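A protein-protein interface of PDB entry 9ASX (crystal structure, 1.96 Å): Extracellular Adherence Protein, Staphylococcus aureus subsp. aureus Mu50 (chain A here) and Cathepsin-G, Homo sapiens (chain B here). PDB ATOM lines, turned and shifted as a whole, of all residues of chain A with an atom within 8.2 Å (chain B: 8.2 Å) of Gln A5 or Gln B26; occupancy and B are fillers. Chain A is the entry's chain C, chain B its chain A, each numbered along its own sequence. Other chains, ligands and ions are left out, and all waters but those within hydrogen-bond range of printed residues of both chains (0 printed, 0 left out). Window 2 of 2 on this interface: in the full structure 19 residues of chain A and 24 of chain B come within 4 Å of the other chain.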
ATOM      1  N   THR A   3     -23.218 -26.686  19.015  1.00  0.00           N
ATOM      2  CA  THR A   3     -23.244 -27.390  17.737  1.00  0.00           C
ATOM      3  C   THR A   3     -21.979 -27.074  16.937  1.00  0.00           C
ATOM      4  O   THR A   3     -21.455 -27.919  16.212  1.00  0.00           O
ATOM      5  CB  THR A   3     -24.487 -27.017  16.901  1.00  0.00           C
ATOM      6  OG1 THR A   3     -24.204 -25.863  16.099  1.00  0.00           O
ATOM      7  CG2 THR A   3     -25.668 -26.705  17.809  1.00  0.00           C
ATOM      8  N   TYR A   4     -21.496 -25.843  17.076  1.00  0.00           N
ATOM      9  CA  TYR A   4     -20.241 -25.426  16.466  1.00  0.00           C
ATOM     10  C   TYR A   4     -19.093 -25.655  17.439  1.00  0.00           C
ATOM     11  O   TYR A   4     -19.184 -25.278  18.612  1.00  0.00           O
ATOM     12  CB  TYR A   4     -20.305 -23.956  16.061  1.00  0.00           C
ATOM     13  CG  TYR A   4     -21.094 -23.735  14.802  1.00  0.00           C
ATOM     14  CD1 TYR A   4     -22.472 -23.570  14.841  1.00  0.00           C
ATOM     15  CD2 TYR A   4     -20.463 -23.706  13.568  1.00  0.00           C
ATOM     16  CE1 TYR A   4     -23.200 -23.376  13.684  1.00  0.00           C
ATOM     17  CE2 TYR A   4     -21.179 -23.502  12.401  1.00  0.00           C
ATOM     18  CZ  TYR A   4     -22.547 -23.339  12.465  1.00  0.00           C
ATOM     19  OH  TYR A   4     -23.264 -23.144  11.307  1.00  0.00           O
ATOM     20  N   GLN A   5     -18.010 -26.251  16.940  1.00  0.00           N
ATOM     21  CA  GLN A   5     -16.847 -26.566  17.756  1.00  0.00           C
ATOM     22  C   GLN A   5     -15.566 -26.246  16.996  1.00  0.00           C
ATOM     23  O   GLN A   5     -15.508 -26.351  15.768  1.00  0.00           O
ATOM     24  CB  GLN A   5     -16.840 -28.035  18.180  1.00  0.00           C
ATOM     25  CG  GLN A   5     -17.920 -28.381  19.195  1.00  0.00           C
ATOM     26  CD  GLN A   5     -17.773 -29.793  19.700  1.00  0.00           C
ATOM     27  OE1 GLN A   5     -17.095 -30.608  19.075  1.00  0.00           O
ATOM     28  NE2 GLN A   5     -18.399 -30.095  20.837  1.00  0.00           N
ATOM     29  N   VAL A   6     -14.540 -25.846  17.749  1.00  0.00           N
ATOM     30  CA  VAL A   6     -13.240 -25.505  17.197  1.00  0.00           C
ATOM     31  C   VAL A   6     -12.182 -26.140  18.087  1.00  0.00           C
ATOM     32  O   VAL A   6     -12.138 -25.859  19.289  1.00  0.00           O
ATOM     33  CB  VAL A   6     -13.014 -23.987  17.112  1.00  0.00           C
ATOM     34  CG1 VAL A   6     -11.586 -23.691  16.644  1.00  0.00           C
ATOM     35  CG2 VAL A   6     -14.050 -23.335  16.177  1.00  0.00           C
ATOM     36  N   PRO A   7     -11.325 -27.002  17.564  1.00  0.00           N
ATOM     37  CA  PRO A   7     -10.275 -27.591  18.401  1.00  0.00           C
ATOM     38  C   PRO A   7      -9.265 -26.541  18.822  1.00  0.00           C
ATOM     39  O   PRO A   7      -8.967 -25.609  18.078  1.00  0.00           O
ATOM     40  CB  PRO A   7      -9.637 -28.648  17.489  1.00  0.00           C
ATOM     41  CG  PRO A   7     -10.031 -28.269  16.107  1.00  0.00           C
ATOM     42  CD  PRO A   7     -11.350 -27.554  16.200  1.00  0.00           C
ATOM     43  N   TYR A   8      -8.755 -26.686  20.044  1.00  0.00           N
ATOM     44  CA  TYR A   8      -7.682 -25.824  20.509  1.00  0.00           C
ATOM     45  C   TYR A   8      -6.675 -26.670  21.268  1.00  0.00           C
ATOM     46  O   TYR A   8      -7.004 -27.735  21.783  1.00  0.00           O
ATOM     47  CB  TYR A   8      -8.192 -24.689  21.411  1.00  0.00           C
ATOM     48  CG  TYR A   8      -8.688 -25.197  22.758  1.00  0.00           C
ATOM     49  CD1 TYR A   8     -10.008 -25.594  22.919  1.00  0.00           C
ATOM     50  CD2 TYR A   8      -7.837 -25.273  23.862  1.00  0.00           C
ATOM     51  CE1 TYR A   8     -10.472 -26.076  24.136  1.00  0.00           C
ATOM     52  CE2 TYR A   8      -8.302 -25.759  25.108  1.00  0.00           C
ATOM     53  CZ  TYR A   8      -9.615 -26.154  25.221  1.00  0.00           C
ATOM     54  OH  TYR A   8     -10.115 -26.617  26.414  1.00  0.00           O
ATOM     55  N   ILE A  19      -4.620 -34.345  25.401  1.00  0.00           N
ATOM     56  CA  ILE A  19      -6.079 -34.337  25.335  1.00  0.00           C
ATOM     57  C   ILE A  19      -6.497 -33.750  23.994  1.00  0.00           C
ATOM     58  O   ILE A  19      -5.764 -32.946  23.398  1.00  0.00           O
ATOM     59  CB  ILE A  19      -6.655 -33.524  26.512  1.00  0.00           C
ATOM     60  CG1 ILE A  19      -8.174 -33.712  26.614  1.00  0.00           C
ATOM     61  CG2 ILE A  19      -6.326 -32.037  26.328  1.00  0.00           C
ATOM     62  CD1 ILE A  19      -8.751 -33.119  27.919  1.00  0.00           C
ATOM     63  N   LEU A  20      -7.664 -34.158  23.490  1.00  0.00           N
ATOM     64  CA  LEU A  20      -8.261 -33.540  22.310  1.00  0.00           C
ATOM     65  C   LEU A  20      -9.418 -32.661  22.778  1.00  0.00           C
ATOM     66  O   LEU A  20     -10.460 -33.177  23.181  1.00  0.00           O
ATOM     67  CB  LEU A  20      -8.735 -34.598  21.318  1.00  0.00           C
ATOM     68  CG  LEU A  20      -9.483 -34.099  20.083  1.00  0.00           C
ATOM     69  CD1 LEU A  20      -8.602 -33.158  19.286  1.00  0.00           C
ATOM     70  CD2 LEU A  20      -9.930 -35.289  19.230  1.00  0.00           C
ATOM     71  N   SER A  21      -9.231 -31.344  22.737  1.00  0.00           N
ATOM     72  CA  SER A  21     -10.180 -30.397  23.313  1.00  0.00           C
ATOM     73  C   SER A  21     -10.756 -29.455  22.261  1.00  0.00           C
ATOM     74  O   SER A  21     -10.091 -29.119  21.279  1.00  0.00           O
ATOM     75  CB  SER A  21      -9.510 -29.570  24.409  1.00  0.00           C
ATOM     76  OG  SER A  21      -9.272 -30.369  25.539  1.00  0.00           O
ATOM     77  N   ASN A  22     -11.992 -28.999  22.507  1.00  0.00           N
ATOM     78  CA  ASN A  22     -12.700 -28.105  21.596  1.00  0.00           C
ATOM     79  C   ASN A  22     -13.435 -27.027  22.373  1.00  0.00           C
ATOM     80  O   ASN A  22     -13.940 -27.273  23.468  1.00  0.00           O
ATOM     81  CB  ASN A  22     -13.746 -28.839  20.755  1.00  0.00           C
ATOM     82  CG  ASN A  22     -13.183 -30.017  20.064  1.00  0.00           C
ATOM     83  OD1 ASN A  22     -12.631 -29.900  18.983  1.00  0.00           O
ATOM     84  ND2 ASN A  22     -13.272 -31.172  20.703  1.00  0.00           N
ATOM     85  N   LEU A  23     -13.502 -25.837  21.782  1.00  0.00           N
ATOM     86  CA  LEU A  23     -14.374 -24.768  22.254  1.00  0.00           C
ATOM     87  C   LEU A  23     -15.735 -24.955  21.608  1.00  0.00           C
ATOM     88  O   LEU A  23     -15.816 -25.183  20.400  1.00  0.00           O
ATOM     89  CB  LEU A  23     -13.841 -23.378  21.885  1.00  0.00           C
ATOM     90  CG  LEU A  23     -12.513 -22.802  22.370  1.00  0.00           C
ATOM     91  CD1 LEU A  23     -12.295 -21.427  21.731  1.00  0.00           C
ATOM     92  CD2 LEU A  23     -12.475 -22.684  23.886  1.00  0.00           C
ATOM     93  N   SER A  24     -16.796 -24.866  22.406  1.00  0.00           N
ATOM     94  CA  SER A  24     -18.139 -24.922  21.853  1.00  0.00           C
ATOM     95  C   SER A  24     -18.663 -23.515  21.596  1.00  0.00           C
ATOM     96  O   SER A  24     -18.460 -22.599  22.398  1.00  0.00           O
ATOM     97  CB  SER A  24     -19.091 -25.672  22.793  1.00  0.00           C
ATOM     98  OG  SER A  24     -20.370 -25.767  22.194  1.00  0.00           O
ATOM     99  N   PHE A  25     -19.302 -23.342  20.446  1.00  0.00           N
ATOM    100  CA  PHE A  25     -20.007 -22.112  20.129  1.00  0.00           C
ATOM    101  C   PHE A  25     -21.512 -22.328  20.062  1.00  0.00           C
ATOM    102  O   PHE A  25     -22.247 -21.431  19.623  1.00  0.00           O
ATOM    103  CB  PHE A  25     -19.469 -21.520  18.824  1.00  0.00           C
ATOM    104  CG  PHE A  25     -18.054 -21.047  18.930  1.00  0.00           C
ATOM    105  CD1 PHE A  25     -17.005 -21.934  18.765  1.00  0.00           C
ATOM    106  CD2 PHE A  25     -17.769 -19.716  19.220  1.00  0.00           C
ATOM    107  CE1 PHE A  25     -15.701 -21.519  18.883  1.00  0.00           C
ATOM    108  CE2 PHE A  25     -16.461 -19.291  19.335  1.00  0.00           C
ATOM    109  CZ  PHE A  25     -15.423 -20.190  19.168  1.00  0.00           C
ATOM    110  N   SER A  26     -21.977 -23.505  20.485  1.00  0.00           N
ATOM    111  CA  SER A  26     -23.392 -23.829  20.691  1.00  0.00           C
ATOM    112  C   SER A  26     -24.149 -23.537  19.404  1.00  0.00           C
ATOM    113  O   SER A  26     -23.776 -24.083  18.352  1.00  0.00           O
ATOM    114  CB  SER A  26     -23.887 -23.084  21.934  1.00  0.00           C
ATOM    115  OG  SER A  26     -23.945 -21.686  21.704  1.00  0.00           O
ATOM    116  N   PRO A  29     -22.723 -19.234  15.906  1.00  0.00           N
ATOM    117  CA  PRO A  29     -21.430 -19.369  15.218  1.00  0.00           C
ATOM    118  C   PRO A  29     -20.706 -18.053  14.985  1.00  0.00           C
ATOM    119  O   PRO A  29     -19.507 -18.070  14.676  1.00  0.00           O
ATOM    120  CB  PRO A  29     -21.819 -20.006  13.884  1.00  0.00           C
ATOM    121  CG  PRO A  29     -23.175 -19.410  13.615  1.00  0.00           C
ATOM    122  CD  PRO A  29     -23.853 -19.355  14.966  1.00  0.00           C
ATOM    123  N   LYS A  68      -9.501 -22.279   7.917  1.00  0.00           N
ATOM    124  CA  LYS A  68      -9.546 -23.475   7.081  1.00  0.00           C
ATOM    125  C   LYS A  68      -9.093 -23.203   5.655  1.00  0.00           C
ATOM    126  O   LYS A  68      -8.605 -24.123   4.987  1.00  0.00           O
ATOM    127  CB  LYS A  68     -10.952 -24.073   7.101  1.00  0.00           C
ATOM    128  CG  LYS A  68     -11.153 -25.020   8.268  1.00  0.00           C
ATOM    129  CD  LYS A  68     -12.515 -24.867   8.914  1.00  0.00           C
ATOM    130  CE  LYS A  68     -13.485 -25.914   8.415  1.00  0.00           C
ATOM    131  NZ  LYS A  68     -14.576 -26.156   9.404  1.00  0.00           N
ATOM    132  N   ALA A  89     -17.467 -19.238  13.155  1.00  0.00           N
ATOM    133  CA  ALA A  89     -16.756 -20.363  13.750  1.00  0.00           C
ATOM    134  C   ALA A  89     -16.435 -21.446  12.731  1.00  0.00           C
ATOM    135  O   ALA A  89     -15.399 -22.105  12.842  1.00  0.00           O
ATOM    136  CB  ALA A  89     -17.571 -20.965  14.895  1.00  0.00           C
ATOM    137  N   LYS A  90     -17.284 -21.628  11.721  1.00  0.00           N
ATOM    138  CA  LYS A  90     -17.069 -22.723  10.776  1.00  0.00           C
ATOM    139  C   LYS A  90     -15.892 -22.465   9.842  1.00  0.00           C
ATOM    140  O   LYS A  90     -15.418 -23.397   9.181  1.00  0.00           O
ATOM    141  CB  LYS A  90     -18.353 -22.972   9.974  1.00  0.00           C
ATOM    142  CG  LYS A  90     -18.282 -24.151   9.021  1.00  0.00           C
ATOM    143  CD  LYS A  90     -19.656 -24.538   8.494  1.00  0.00           C
ATOM    144  CE  LYS A  90     -19.590 -25.787   7.613  1.00  0.00           C
ATOM    145  NZ  LYS A  90     -19.724 -27.043   8.408  1.00  0.00           N
ATOM    146  N   ASP A  91     -15.396 -21.232   9.791  1.00  0.00           N
ATOM    147  CA  ASP A  91     -14.212 -20.907   9.015  1.00  0.00           C
ATOM    148  C   ASP A  91     -12.913 -21.202   9.751  1.00  0.00           C
ATOM    149  O   ASP A  91     -11.843 -21.124   9.138  1.00  0.00           O
ATOM    150  CB  ASP A  91     -14.230 -19.425   8.623  1.00  0.00           C
ATOM    151  CG  ASP A  91     -15.290 -19.107   7.578  1.00  0.00           C
ATOM    152  OD1 ASP A  91     -15.544 -19.967   6.702  1.00  0.00           O
ATOM    153  OD2 ASP A  91     -15.859 -17.985   7.635  1.00  0.00           O
ATOM    154  N   VAL A  92     -12.966 -21.509  11.042  1.00  0.00           N
ATOM    155  CA  VAL A  92     -11.753 -21.701  11.826  1.00  0.00           C
ATOM    156  C   VAL A  92     -11.371 -23.174  11.829  1.00  0.00           C
ATOM    157  O   VAL A  92     -12.194 -24.037  12.144  1.00  0.00           O
ATOM    158  CB  VAL A  92     -11.936 -21.186  13.260  1.00  0.00           C
ATOM    159  CG1 VAL A  92     -10.698 -21.535  14.082  1.00  0.00           C
ATOM    160  CG2 VAL A  92     -12.225 -19.677  13.267  1.00  0.00           C
ATOM    161  N   LYS A  93     -10.107 -23.456  11.510  1.00  0.00           N
ATOM    162  CA  LYS A  93      -9.591 -24.821  11.552  1.00  0.00           C
ATOM    163  C   LYS A  93      -9.222 -25.250  12.970  1.00  0.00           C
ATOM    164  O   LYS A  93      -9.673 -26.300  13.441  1.00  0.00           O
ATOM    165  CB  LYS A  93      -8.377 -24.946  10.629  1.00  0.00           C
ATOM    166  CG  LYS A  93      -7.808 -26.360  10.549  1.00  0.00           C
ATOM    167  CD  LYS A  93      -6.632 -26.476   9.590  1.00  0.00           C
ATOM    168  CE  LYS A  93      -6.089 -27.907   9.569  1.00  0.00           C
ATOM    169  NZ  LYS A  93      -4.934 -28.066   8.641  1.00  0.00           N
ATOM    170  N   ARG A  94      -8.405 -24.456  13.665  1.00  0.00           N
ATOM    171  CA  ARG A  94      -7.941 -24.802  15.002  1.00  0.00           C
ATOM    172  C   ARG A  94      -7.393 -23.544  15.657  1.00  0.00           C
ATOM    173  O   ARG A  94      -7.110 -22.551  14.992  1.00  0.00           O
ATOM    174  CB  ARG A  94      -6.869 -25.889  14.967  1.00  0.00           C
ATOM    175  CG  ARG A  94      -5.672 -25.527  14.101  1.00  0.00           C
ATOM    176  CD  ARG A  94      -4.828 -26.759  13.781  1.00  0.00           C
ATOM    177  NE  ARG A  94      -3.691 -26.851  14.682  1.00  0.00           N
ATOM    178  CZ  ARG A  94      -2.494 -26.347  14.425  1.00  0.00           C
ATOM    179  NH1 ARG A  94      -2.208 -25.816  13.244  1.00  0.00           N
ATOM    180  NH2 ARG A  94      -1.566 -26.364  15.375  1.00  0.00           N
ATOM    181  N   LEU B  18     -13.382 -41.801  26.191  1.00  0.00           N
ATOM    182  CA  LEU B  18     -14.051 -40.884  27.104  1.00  0.00           C
ATOM    183  C   LEU B  18     -14.537 -39.645  26.365  1.00  0.00           C
ATOM    184  O   LEU B  18     -13.768 -39.020  25.637  1.00  0.00           O
ATOM    185  CB  LEU B  18     -13.120 -40.460  28.239  1.00  0.00           C
ATOM    186  CG  LEU B  18     -12.394 -41.518  29.070  1.00  0.00           C
ATOM    187  CD1 LEU B  18     -11.598 -40.869  30.223  1.00  0.00           C
ATOM    188  CD2 LEU B  18     -13.361 -42.541  29.596  1.00  0.00           C
ATOM    189  N   GLN B  19     -15.809 -39.298  26.563  1.00  0.00           N
ATOM    190  CA  GLN B  19     -16.403 -38.059  26.072  1.00  0.00           C
ATOM    191  C   GLN B  19     -16.675 -37.168  27.275  1.00  0.00           C
ATOM    192  O   GLN B  19     -17.411 -37.556  28.184  1.00  0.00           O
ATOM    193  CB  GLN B  19     -17.696 -38.324  25.297  1.00  0.00           C
ATOM    194  CG  GLN B  19     -17.505 -39.282  24.131  1.00  0.00           C
ATOM    195  CD  GLN B  19     -18.808 -39.638  23.470  1.00  0.00           C
ATOM    196  OE1 GLN B  19     -19.151 -39.097  22.418  1.00  0.00           O
ATOM    197  NE2 GLN B  19     -19.554 -40.551  24.091  1.00  0.00           N
ATOM    198  N   ILE B  20     -16.103 -35.970  27.262  1.00  0.00           N
ATOM    199  CA  ILE B  20     -15.978 -35.135  28.446  1.00  0.00           C
ATOM    200  C   ILE B  20     -16.645 -33.800  28.152  1.00  0.00           C
ATOM    201  O   ILE B  20     -16.352 -33.174  27.127  1.00  0.00           O
ATOM    202  CB  ILE B  20     -14.500 -34.924  28.836  1.00  0.00           C
ATOM    203  CG1 ILE B  20     -13.815 -36.271  29.142  1.00  0.00           C
ATOM    204  CG2 ILE B  20     -14.368 -33.912  30.001  1.00  0.00           C
ATOM    205  CD1 ILE B  20     -12.453 -36.397  28.468  1.00  0.00           C
ATOM    206  N   GLN B  21     -17.518 -33.365  29.059  1.00  0.00           N
ATOM    207  CA  GLN B  21     -18.141 -32.049  28.998  1.00  0.00           C
ATOM    208  C   GLN B  21     -17.423 -31.092  29.934  1.00  0.00           C
ATOM    209  O   GLN B  21     -17.197 -31.414  31.102  1.00  0.00           O
ATOM    210  CB  GLN B  21     -19.614 -32.115  29.382  1.00  0.00           C
ATOM    211  CG  GLN B  21     -20.545 -32.197  28.194  1.00  0.00           C
ATOM    212  CD  GLN B  21     -20.644 -30.896  27.436  1.00  0.00           C
ATOM    213  OE1 GLN B  21     -20.287 -29.834  27.950  1.00  0.00           O
ATOM    214  NE2 GLN B  21     -21.128 -30.968  26.204  1.00  0.00           N
ATOM    215  N   SER B  22     -17.082 -29.917  29.428  1.00  0.00           N
ATOM    216  CA  SER B  22     -16.359 -28.893  30.171  1.00  0.00           C
ATOM    217  C   SER B  22     -17.113 -27.579  30.051  1.00  0.00           C
ATOM    218  O   SER B  22     -18.057 -27.465  29.260  1.00  0.00           O
ATOM    219  CB  SER B  22     -14.917 -28.763  29.641  1.00  0.00           C
ATOM    220  OG  SER B  22     -14.872 -28.018  28.434  1.00  0.00           O
ATOM    221  N   PRO B  23     -16.746 -26.566  30.847  1.00  0.00           N
ATOM    222  CA  PRO B  23     -17.415 -25.256  30.703  1.00  0.00           C
ATOM    223  C   PRO B  23     -17.401 -24.716  29.282  1.00  0.00           C
ATOM    224  O   PRO B  23     -18.451 -24.340  28.746  1.00  0.00           O
ATOM    225  CB  PRO B  23     -16.619 -24.359  31.662  1.00  0.00           C
ATOM    226  CG  PRO B  23     -16.063 -25.288  32.669  1.00  0.00           C
ATOM    227  CD  PRO B  23     -15.795 -26.577  31.973  1.00  0.00           C
ATOM    228  N   ALA B  24     -16.240 -24.716  28.637  1.00  0.00           N
ATOM    229  CA  ALA B  24     -16.081 -24.087  27.339  1.00  0.00           C
ATOM    230  C   ALA B  24     -16.398 -25.000  26.163  1.00  0.00           C
ATOM    231  O   ALA B  24     -16.564 -24.489  25.051  1.00  0.00           O
ATOM    232  CB  ALA B  24     -14.659 -23.552  27.186  1.00  0.00           C
ATOM    233  N   GLY B  25     -16.468 -26.313  26.370  1.00  0.00           N
ATOM    234  CA  GLY B  25     -16.734 -27.204  25.253  1.00  0.00           C
ATOM    235  C   GLY B  25     -16.617 -28.670  25.633  1.00  0.00           C
ATOM    236  O   GLY B  25     -16.925 -29.063  26.758  1.00  0.00           O
ATOM    237  N   GLN B  26     -16.129 -29.460  24.680  1.00  0.00           N
ATOM    238  CA  GLN B  26     -16.047 -30.907  24.812  1.00  0.00           C
ATOM    239  C   GLN B  26     -14.626 -31.392  24.575  1.00  0.00           C
ATOM    240  O   GLN B  26     -13.881 -30.813  23.787  1.00  0.00           O
ATOM    241  CB  GLN B  26     -16.972 -31.584  23.821  1.00  0.00           C
ATOM    242  CG  GLN B  26     -18.400 -31.540  24.245  1.00  0.00           C
ATOM    243  CD  GLN B  26     -19.140 -32.723  23.721  1.00  0.00           C
ATOM    244  OE1 GLN B  26     -19.394 -33.691  24.449  1.00  0.00           O
ATOM    245  NE2 GLN B  26     -19.476 -32.678  22.436  1.00  0.00           N
ATOM    246  N   SER B  27     -14.260 -32.488  25.242  1.00  0.00           N
ATOM    247  CA  SER B  27     -12.945 -33.086  25.071  1.00  0.00           C
ATOM    248  C   SER B  27     -13.090 -34.592  24.879  1.00  0.00           C
ATOM    249  O   SER B  27     -14.142 -35.177  25.149  1.00  0.00           O
ATOM    250  CB  SER B  27     -12.029 -32.796  26.275  1.00  0.00           C
ATOM    251  OG  SER B  27     -11.713 -31.401  26.368  1.00  0.00           O
ATOM    252  N   ARG B  28     -12.011 -35.211  24.398  1.00  0.00           N
ATOM    253  CA  ARG B  28     -11.931 -36.649  24.183  1.00  0.00           C
ATOM    254  C   ARG B  28     -10.606 -37.130  24.745  1.00  0.00           C
ATOM    255  O   ARG B  28      -9.582 -36.463  24.582  1.00  0.00           O
ATOM    256  CB  ARG B  28     -12.034 -36.997  22.700  1.00  0.00           C
ATOM    257  CG  ARG B  28     -13.326 -36.512  22.053  1.00  0.00           C
ATOM    258  CD  ARG B  28     -14.502 -37.256  22.671  1.00  0.00           C
ATOM    259  NE  ARG B  28     -15.773 -36.910  22.037  1.00  0.00           N
ATOM    260  CZ  ARG B  28     -16.593 -35.951  22.452  1.00  0.00           C
ATOM    261  NH1 ARG B  28     -16.325 -35.221  23.526  1.00  0.00           N
ATOM    262  NH2 ARG B  28     -17.716 -35.721  21.776  1.00  0.00           N
ATOM    263  N   CYS B  29     -10.644 -38.286  25.400  1.00  0.00           N
ATOM    264  CA  CYS B  29      -9.486 -38.905  26.028  1.00  0.00           C
ATOM    265  C   CYS B  29      -9.627 -40.415  25.898  1.00  0.00           C
ATOM    266  O   CYS B  29     -10.683 -40.934  25.521  1.00  0.00           O
ATOM    267  CB  CYS B  29      -9.382 -38.547  27.529  1.00  0.00           C
ATOM    268  SG  CYS B  29      -8.631 -36.937  27.886  1.00  0.00           S
ATOM    269  N   ASN B  49     -19.169 -33.716  33.289  1.00  0.00           N
ATOM    270  CA  ASN B  49     -19.902 -34.897  32.841  1.00  0.00           C
ATOM    271  C   ASN B  49     -18.988 -35.702  31.945  1.00  0.00           C
ATOM    272  O   ASN B  49     -18.374 -35.133  31.037  1.00  0.00           O
ATOM    273  CB  ASN B  49     -21.169 -34.512  32.071  1.00  0.00           C
ATOM    274  CG  ASN B  49     -22.125 -33.698  32.910  1.00  0.00           C
ATOM    275  OD1 ASN B  49     -22.854 -34.245  33.737  1.00  0.00           O
ATOM    276  ND2 ASN B  49     -22.122 -32.382  32.710  1.00  0.00           N
ATOM    277  N   ASN B  51     -18.832 -39.454  29.752  1.00  0.00           N
ATOM    278  CA  ASN B  51     -19.415 -40.693  29.239  1.00  0.00           C
ATOM    279  C   ASN B  51     -18.292 -41.629  28.836  1.00  0.00           C
ATOM    280  O   ASN B  51     -17.365 -41.222  28.128  1.00  0.00           O
ATOM    281  CB  ASN B  51     -20.306 -40.443  28.025  1.00  0.00           C
ATOM    282  CG  ASN B  51     -21.617 -39.818  28.382  1.00  0.00           C
ATOM    283  OD1 ASN B  51     -22.089 -39.893  29.520  1.00  0.00           O
ATOM    284  ND2 ASN B  51     -22.228 -39.191  27.398  1.00  0.00           N
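The backbone NH (N) of Asn A22 lies within hydrogen-bond range of the backbone carbonyl oxygen (O) of Gln B26, at 2.9 Å.
OG of Ser B27 is in hydrogen-bond range of OG of Ser A21, 2.8 Å away.
The backbone NH (N) of Ser A24 lies within hydrogen-bond range of the backbone carbonyl oxygen (O) of Ala B24.
The side-chain amide nitrogen (NE2) of Gln B26 sits close to the side-chain amide nitrogen (NE2) of Gln A5, at 3.2 Å.
The backbone NH (N) of Arg B28 lies within hydrogen-bond range of the backbone carbonyl oxygen (O) of Leu A20 (2.8 Å).
The backbone NH of Leu B18 is in hydrogen-bond range of the backbone carbonyl oxygen of Cys B29 (2.9 Å).
The side-chain hydroxyl (OG) of Ser B22 is in hydrogen-bond range of the backbone carbonyl oxygen (O) of Gly B25 (2.8 Å).
The backbone carbonyl oxygen (O) of Ile B20 is in hydrogen-bond range of the backbone NH (N) of Ser B27 (2.9 Å).
OG of Ser A24 is in hydrogen-bond range of N of Ser A26.
O of Val A6 is in hydrogen-bond range of N of Leu A23, at 2.8 Å.
O of Ser A21 is in hydrogen-bond range of N of Tyr A8 (3.0 Å).
CD1 of Ile A19 touches CB of Ser B27, at 3.7 Å.
CG1 of Ile A19 touches O of Arg B28 (3.7 Å).
Cys B29 touches Ile A19 (SG to CG1, 3.5 Å).
CA of Ser B27 touches O of Leu A20, 3.1 Å away.
Ser A21 touches Gln B26 (C to O, 3.7 Å).
Asn A22 touches Gly B25.
Ala B24 touches Leu A23.
Gly B25 touches Ser A24 (CA to N, 3.7 Å).
Tyr A4 touches none of the printed residues of chain B.
Printed residues of chain B within 4 Å of Gln A5: Gln B26 (3.2 Å).
Of the printed residues of chain B, Leu A20 touches Ser B27 (3.1 Å) and Arg B28 (2.8 Å).
Printed residues of chain B within 4 Å of Ser A21: Gln B26 (3.7 Å) and Ser B27 (2.8 Å).
Printed residues of chain B within 4 Å of Asn A22: Gly B25 and Gln B26.
Of the printed residues of chain B, Leu A23 touches Ala B24.
Ile B20 touches none of the printed residues of chain A.
Of the printed residues of chain A, Ala B24 touches Leu A23 (3.6 Å) and Ser A24 (2.7 Å).
Gly B25 touches two residues of chain A.
Ser B27 touches just these residues of chain A: Ile A19, Leu A20 and Ser A21.
The nearest residue of chain A that does not touch Gln B26 is Leu A20 (4.2 Å).
The nearest printed residue of chain A that does not touch Ala B24 is Asn A22 (4.1 Å).
Of the 14 printed residues of chain B, 6 touch a printed residue of chain A.
Printed residues of chain B that touch a printed residue of chain A: Ala B24, Gly B25, Gln B26, Ser B27, Arg B28 and Cys B29.
Hydrophobic or aromatic side chains of chain A within 4 Å of the printed part of chain B: Ile A19 and Leu A20.
Among the printed residues, 13 pairs touch across the chains.
Among the printed residues, no Asp or Glu carboxylate lies within 4 Å of a Lys or Arg side-chain nitrogen of the other chain.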
